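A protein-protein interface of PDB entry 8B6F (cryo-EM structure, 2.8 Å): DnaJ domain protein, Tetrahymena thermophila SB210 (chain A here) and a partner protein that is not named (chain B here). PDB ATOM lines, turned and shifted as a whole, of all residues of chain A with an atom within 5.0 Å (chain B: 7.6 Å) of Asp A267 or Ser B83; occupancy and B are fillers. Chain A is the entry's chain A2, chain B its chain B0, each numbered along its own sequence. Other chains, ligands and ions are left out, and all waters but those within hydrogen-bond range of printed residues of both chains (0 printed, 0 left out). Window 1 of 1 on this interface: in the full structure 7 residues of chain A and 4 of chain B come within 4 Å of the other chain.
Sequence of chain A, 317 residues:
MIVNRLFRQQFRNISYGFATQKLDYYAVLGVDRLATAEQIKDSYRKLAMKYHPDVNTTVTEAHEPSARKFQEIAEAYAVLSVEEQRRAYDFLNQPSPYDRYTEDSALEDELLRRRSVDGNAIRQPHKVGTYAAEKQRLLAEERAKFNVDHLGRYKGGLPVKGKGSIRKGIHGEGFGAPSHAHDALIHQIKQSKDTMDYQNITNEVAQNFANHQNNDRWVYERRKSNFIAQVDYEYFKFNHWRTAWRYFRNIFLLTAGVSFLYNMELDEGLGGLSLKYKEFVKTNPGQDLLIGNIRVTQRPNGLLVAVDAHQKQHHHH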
ATOM      1  N   PHE A 260      20.995  34.057 -25.696  1.00  0.00           N
ATOM      2  CA  PHE A 260      20.073  32.928 -25.678  1.00  0.00           C
ATOM      3  C   PHE A 260      20.542  31.809 -26.597  1.00  0.00           C
ATOM      4  O   PHE A 260      20.491  30.632 -26.226  1.00  0.00           O
ATOM      5  CB  PHE A 260      18.674  33.381 -26.084  1.00  0.00           C
ATOM      6  CG  PHE A 260      17.823  32.271 -26.625  1.00  0.00           C
ATOM      7  CD1 PHE A 260      17.176  31.396 -25.772  1.00  0.00           C
ATOM      8  CD2 PHE A 260      17.680  32.099 -27.991  1.00  0.00           C
ATOM      9  CE1 PHE A 260      16.399  30.371 -26.271  1.00  0.00           C
ATOM     10  CE2 PHE A 260      16.906  31.078 -28.496  1.00  0.00           C
ATOM     11  CZ  PHE A 260      16.264  30.213 -27.636  1.00  0.00           C
ATOM     12  N   ASN A 263      23.570  30.062 -24.975  1.00  0.00           N
ATOM     13  CA  ASN A 263      23.166  29.300 -23.798  1.00  0.00           C
ATOM     14  C   ASN A 263      22.331  28.088 -24.189  1.00  0.00           C
ATOM     15  O   ASN A 263      22.482  27.009 -23.606  1.00  0.00           O
ATOM     16  CB  ASN A 263      22.390  30.194 -22.833  1.00  0.00           C
ATOM     17  CG  ASN A 263      23.211  31.365 -22.334  1.00  0.00           C
ATOM     18  OD1 ASN A 263      24.426  31.264 -22.180  1.00  0.00           O
ATOM     19  ND2 ASN A 263      22.546  32.484 -22.072  1.00  0.00           N
ATOM     20  N   MET A 264      21.449  28.246 -25.177  1.00  0.00           N
ATOM     21  CA  MET A 264      20.650  27.119 -25.642  1.00  0.00           C
ATOM     22  C   MET A 264      21.530  26.037 -26.246  1.00  0.00           C
ATOM     23  O   MET A 264      21.309  24.843 -26.014  1.00  0.00           O
ATOM     24  CB  MET A 264      19.614  27.597 -26.658  1.00  0.00           C
ATOM     25  CG  MET A 264      18.724  26.489 -27.210  1.00  0.00           C
ATOM     26  SD  MET A 264      17.520  27.109 -28.399  1.00  0.00           S
ATOM     27  CE  MET A 264      16.609  25.616 -28.780  1.00  0.00           C
ATOM     28  N   GLU A 265      22.538  26.432 -27.025  1.00  0.00           N
ATOM     29  CA  GLU A 265      23.453  25.448 -27.589  1.00  0.00           C
ATOM     30  C   GLU A 265      24.213  24.715 -26.492  1.00  0.00           C
ATOM     31  O   GLU A 265      24.387  23.493 -26.557  1.00  0.00           O
ATOM     32  CB  GLU A 265      24.417  26.137 -28.553  1.00  0.00           C
ATOM     33  CG  GLU A 265      25.163  25.188 -29.469  1.00  0.00           C
ATOM     34  CD  GLU A 265      24.241  24.441 -30.409  1.00  0.00           C
ATOM     35  OE1 GLU A 265      23.051  24.806 -30.494  1.00  0.00           O
ATOM     36  OE2 GLU A 265      24.708  23.488 -31.066  1.00  0.00           O
ATOM     37  N   LEU A 266      24.681  25.444 -25.476  1.00  0.00           N
ATOM     38  CA  LEU A 266      25.372  24.794 -24.367  1.00  0.00           C
ATOM     39  C   LEU A 266      24.456  23.816 -23.648  1.00  0.00           C
ATOM     40  O   LEU A 266      24.860  22.692 -23.330  1.00  0.00           O
ATOM     41  CB  LEU A 266      25.902  25.833 -23.381  1.00  0.00           C
ATOM     42  CG  LEU A 266      27.084  26.699 -23.808  1.00  0.00           C
ATOM     43  CD1 LEU A 266      27.407  27.663 -22.683  1.00  0.00           C
ATOM     44  CD2 LEU A 266      28.299  25.864 -24.172  1.00  0.00           C
ATOM     45  N   ASP A 267      23.213  24.224 -23.389  1.00  0.00           N
ATOM     46  CA  ASP A 267      22.280  23.349 -22.687  1.00  0.00           C
ATOM     47  C   ASP A 267      21.971  22.110 -23.514  1.00  0.00           C
ATOM     48  O   ASP A 267      21.890  20.999 -22.976  1.00  0.00           O
ATOM     49  CB  ASP A 267      20.996  24.109 -22.360  1.00  0.00           C
ATOM     50  CG  ASP A 267      21.249  25.340 -21.511  1.00  0.00           C
ATOM     51  OD1 ASP A 267      22.424  25.607 -21.185  1.00  0.00           O
ATOM     52  OD2 ASP A 267      20.272  26.040 -21.168  1.00  0.00           O
ATOM     53  N   GLU A 268      21.790  22.279 -24.823  1.00  0.00           N
ATOM     54  CA  GLU A 268      21.563  21.127 -25.687  1.00  0.00           C
ATOM     55  C   GLU A 268      22.757  20.179 -25.656  1.00  0.00           C
ATOM     56  O   GLU A 268      22.586  18.956 -25.597  1.00  0.00           O
ATOM     57  CB  GLU A 268      21.284  21.595 -27.115  1.00  0.00           C
ATOM     58  CG  GLU A 268      20.943  20.478 -28.083  1.00  0.00           C
ATOM     59  CD  GLU A 268      20.783  20.977 -29.505  1.00  0.00           C
ATOM     60  OE1 GLU A 268      20.929  22.196 -29.725  1.00  0.00           O
ATOM     61  OE2 GLU A 268      20.517  20.151 -30.403  1.00  0.00           O
ATOM     62  N   GLY A 269      23.973  20.725 -25.702  1.00  0.00           N
ATOM     63  CA  GLY A 269      25.152  19.877 -25.631  1.00  0.00           C
ATOM     64  C   GLY A 269      25.258  19.126 -24.318  1.00  0.00           C
ATOM     65  O   GLY A 269      25.579  17.937 -24.296  1.00  0.00           O
ATOM     66  N   LEU A 270      24.989  19.811 -23.205  1.00  0.00           N
ATOM     67  CA  LEU A 270      25.056  19.155 -21.903  1.00  0.00           C
ATOM     68  C   LEU A 270      24.008  18.057 -21.790  1.00  0.00           C
ATOM     69  O   LEU A 270      24.290  16.969 -21.276  1.00  0.00           O
ATOM     70  CB  LEU A 270      24.884  20.183 -20.786  1.00  0.00           C
ATOM     71  CG  LEU A 270      25.997  21.227 -20.671  1.00  0.00           C
ATOM     72  CD1 LEU A 270      25.618  22.295 -19.662  1.00  0.00           C
ATOM     73  CD2 LEU A 270      27.317  20.578 -20.289  1.00  0.00           C
ATOM     74  N   GLY A 271      22.788  18.330 -22.252  1.00  0.00           N
ATOM     75  CA  GLY A 271      21.762  17.302 -22.237  1.00  0.00           C
ATOM     76  C   GLY A 271      22.117  16.121 -23.119  1.00  0.00           C
ATOM     77  O   GLY A 271      21.906  14.967 -22.742  1.00  0.00           O
ATOM     78  N   GLY A 272      22.676  16.393 -24.298  1.00  0.00           N
ATOM     79  CA  GLY A 272      23.107  15.308 -25.164  1.00  0.00           C
ATOM     80  C   GLY A 272      24.182  14.452 -24.523  1.00  0.00           C
ATOM     81  O   GLY A 272      24.138  13.223 -24.598  1.00  0.00           O
ATOM     82  N   PRO B  78      21.920  21.539 -14.573  1.00  0.00           N
ATOM     83  CA  PRO B  78      22.408  22.789 -15.178  1.00  0.00           C
ATOM     84  C   PRO B  78      21.694  23.147 -16.465  1.00  0.00           C
ATOM     85  O   PRO B  78      21.601  24.333 -16.803  1.00  0.00           O
ATOM     86  CB  PRO B  78      23.899  22.509 -15.415  1.00  0.00           C
ATOM     87  CG  PRO B  78      24.235  21.393 -14.495  1.00  0.00           C
ATOM     88  CD  PRO B  78      23.002  20.557 -14.399  1.00  0.00           C
ATOM     89  N   TRP B  79      21.177  22.158 -17.188  1.00  0.00           N
ATOM     90  CA  TRP B  79      20.550  22.377 -18.482  1.00  0.00           C
ATOM     91  C   TRP B  79      19.027  22.370 -18.409  1.00  0.00           C
ATOM     92  O   TRP B  79      18.367  22.417 -19.451  1.00  0.00           O
ATOM     93  CB  TRP B  79      21.046  21.333 -19.490  1.00  0.00           C
ATOM     94  CG  TRP B  79      21.210  19.949 -18.932  1.00  0.00           C
ATOM     95  CD1 TRP B  79      22.268  19.479 -18.209  1.00  0.00           C
ATOM     96  CD2 TRP B  79      20.295  18.855 -19.059  1.00  0.00           C
ATOM     97  NE1 TRP B  79      22.067  18.162 -17.876  1.00  0.00           N
ATOM     98  CE2 TRP B  79      20.863  17.755 -18.386  1.00  0.00           C
ATOM     99  CE3 TRP B  79      19.050  18.699 -19.675  1.00  0.00           C
ATOM    100  CZ2 TRP B  79      20.229  16.518 -18.310  1.00  0.00           C
ATOM    101  CZ3 TRP B  79      18.422  17.471 -19.600  1.00  0.00           C
ATOM    102  CH2 TRP B  79      19.013  16.395 -18.923  1.00  0.00           C
ATOM    103  N   TYR B  80      18.453  22.302 -17.203  1.00  0.00           N
ATOM    104  CA  TYR B  80      17.007  22.436 -17.059  1.00  0.00           C
ATOM    105  C   TYR B  80      16.543  23.880 -17.174  1.00  0.00           C
ATOM    106  O   TYR B  80      15.448  24.131 -17.689  1.00  0.00           O
ATOM    107  CB  TYR B  80      16.535  21.856 -15.724  1.00  0.00           C
ATOM    108  CG  TYR B  80      16.474  20.348 -15.682  1.00  0.00           C
ATOM    109  CD1 TYR B  80      16.811  19.588 -16.792  1.00  0.00           C
ATOM    110  CD2 TYR B  80      16.028  19.687 -14.547  1.00  0.00           C
ATOM    111  CE1 TYR B  80      16.738  18.222 -16.767  1.00  0.00           C
ATOM    112  CE2 TYR B  80      15.951  18.310 -14.512  1.00  0.00           C
ATOM    113  CZ  TYR B  80      16.298  17.587 -15.636  1.00  0.00           C
ATOM    114  OH  TYR B  80      16.238  16.219 -15.650  1.00  0.00           O
ATOM    115  N   ASN B  81      17.338  24.832 -16.701  1.00  0.00           N
ATOM    116  CA  ASN B  81      16.915  26.223 -16.727  1.00  0.00           C
ATOM    117  C   ASN B  81      16.744  26.706 -18.159  1.00  0.00           C
ATOM    118  O   ASN B  81      17.525  26.360 -19.049  1.00  0.00           O
ATOM    119  CB  ASN B  81      17.930  27.101 -15.996  1.00  0.00           C
ATOM    120  CG  ASN B  81      18.040  26.757 -14.529  1.00  0.00           C
ATOM    121  OD1 ASN B  81      18.920  26.001 -14.121  1.00  0.00           O
ATOM    122  ND2 ASN B  81      17.137  27.306 -13.724  1.00  0.00           N
ATOM    123  N   THR B  82      15.708  27.509 -18.378  1.00  0.00           N
ATOM    124  CA  THR B  82      15.474  28.080 -19.696  1.00  0.00           C
ATOM    125  C   THR B  82      16.501  29.167 -19.989  1.00  0.00           C
ATOM    126  O   THR B  82      16.847  29.970 -19.119  1.00  0.00           O
ATOM    127  CB  THR B  82      14.056  28.647 -19.788  1.00  0.00           C
ATOM    128  OG1 THR B  82      13.801  29.087 -21.128  1.00  0.00           O
ATOM    129  CG2 THR B  82      13.866  29.814 -18.826  1.00  0.00           C
ATOM    130  N   SER B  83      16.994  29.182 -21.228  1.00  0.00           N
ATOM    131  CA  SER B  83      18.009  30.154 -21.612  1.00  0.00           C
ATOM    132  C   SER B  83      17.453  31.567 -21.709  1.00  0.00           C
ATOM    133  O   SER B  83      18.231  32.525 -21.745  1.00  0.00           O
ATOM    134  CB  SER B  83      18.629  29.755 -22.950  1.00  0.00           C
ATOM    135  OG  SER B  83      19.197  28.460 -22.877  1.00  0.00           O
ATOM    136  N   THR B  84      16.132  31.715 -21.751  1.00  0.00           N
ATOM    137  CA  THR B  84      15.496  33.021 -21.854  1.00  0.00           C
ATOM    138  C   THR B  84      15.344  33.713 -20.507  1.00  0.00           C
ATOM    139  O   THR B  84      14.827  34.835 -20.464  1.00  0.00           O
ATOM    140  CB  THR B  84      14.124  32.881 -22.518  1.00  0.00           C
ATOM    141  OG1 THR B  84      13.317  31.963 -21.772  1.00  0.00           O
ATOM    142  CG2 THR B  84      14.271  32.379 -23.943  1.00  0.00           C
ATOM    143  N   ASN B  85      15.770  33.078 -19.415  1.00  0.00           N
ATOM    144  CA  ASN B  85      15.676  33.658 -18.076  1.00  0.00           C
ATOM    145  C   ASN B  85      14.225  33.853 -17.642  1.00  0.00           C
ATOM    146  O   ASN B  85      13.925  34.711 -16.808  1.00  0.00           O
ATOM    147  CB  ASN B  85      16.438  34.983 -17.991  1.00  0.00           C
ATOM    148  CG  ASN B  85      17.916  34.824 -18.282  1.00  0.00           C
ATOM    149  OD1 ASN B  85      18.522  33.809 -17.940  1.00  0.00           O
ATOM    150  ND2 ASN B  85      18.505  35.830 -18.916  1.00  0.00           N
ATOM    151  N   ASN B  86      13.314  33.062 -18.205  1.00  0.00           N
ATOM    152  CA  ASN B  86      11.912  33.067 -17.786  1.00  0.00           C
ATOM    153  C   ASN B  86      11.673  31.979 -16.738  1.00  0.00           C
ATOM    154  O   ASN B  86      10.855  31.073 -16.903  1.00  0.00           O
ATOM    155  CB  ASN B  86      10.997  32.885 -18.990  1.00  0.00           C
ATOM    156  CG  ASN B  86      10.986  34.094 -19.900  1.00  0.00           C
ATOM    157  OD1 ASN B  86      11.766  34.182 -20.847  1.00  0.00           O
ATOM    158  ND2 ASN B  86      10.094  35.038 -19.617  1.00  0.00           N
ATOM    159  N   ASN B  87      12.420  32.079 -15.645  1.00  0.00           N
ATOM    160  CA  ASN B  87      12.328  31.116 -14.560  1.00  0.00           C
ATOM    161  C   ASN B  87      11.309  31.576 -13.521  1.00  0.00           C
ATOM    162  O   ASN B  87      10.835  32.713 -13.530  1.00  0.00           O
ATOM    163  CB  ASN B  87      13.697  30.917 -13.910  1.00  0.00           C
ATOM    164  CG  ASN B  87      14.740  30.432 -14.894  1.00  0.00           C
ATOM    165  OD1 ASN B  87      14.877  29.232 -15.129  1.00  0.00           O
ATOM    166  ND2 ASN B  87      15.487  31.365 -15.474  1.00  0.00           N
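The side-chain carboxylate (OD2) of Asp A267 lies within hydrogen-bond range of the side-chain hydroxyl (OG) of Ser B83 (3.2 Å). The side-chain carboxylate (OD2) of Asp A267 sits close to the backbone carbonyl oxygen (O) of Asn B81, at 3.5 Å. N of Met A264 sits at hydrogen-bond distance from OG of Ser B83 (3.2 Å).
The side-chain hydroxyl (OG1) of Thr B84 lies within hydrogen-bond range of the side-chain amide oxygen (OD1) of Asn B86. The side-chain amide nitrogen of Asn B81 is in hydrogen-bond range of the side-chain amide oxygen of Asn B87. The side-chain hydroxyl of Thr B82 sits at hydrogen-bond distance from the side-chain hydroxyl of Thr B84, at 3.0 Å.
CD1 of Phe A260 touches CB of Ser B83, at 3.6 Å. Phe A260 touches Thr B84. Asn A263 touches Ser B83 (C to OG, 3.4 Å). Asp A267 touches Trp B79. CD1 of Trp B79 touches CB of Leu A270, at 3.7 Å. Trp B79 touches Gly A271 (CD2 to CA, 3.8 Å).
Of chain B, only Trp B79 (3.6 Å), Asn B81 (3.5 Å) and Ser B83 (3.2 Å) come within 4 Å of Asp A267. Ser B83 touches four residues of chain A. Printed residues of chain B within 4 Å of Met A264: Ser B83 (3.2 Å). Printed residues of chain B within 4 Å of Leu A270: Trp B79. Of the printed residues of chain B, Phe A260 touches Ser B83 (3.6 Å) and Thr B84 (3.6 Å). Glu A265 touches none of the printed residues of chain B. The nearest residue of chain B that does not touch Asp A267 is Pro B78 (4.6 Å). The nearest printed residue of chain A that does not touch Ser B83 is Glu A265 (5.7 Å). The nearest printed residue of chain B that does not touch Asn A263 is Asn B85 (5.9 Å).
Hydrophobic or aromatic side chains of chain A within 4 Å of the printed part of chain B: Phe A260, Met A264 and Leu A270. Hydrophobic or aromatic side chains of chain B that line the printed part of chain A: Trp B79.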
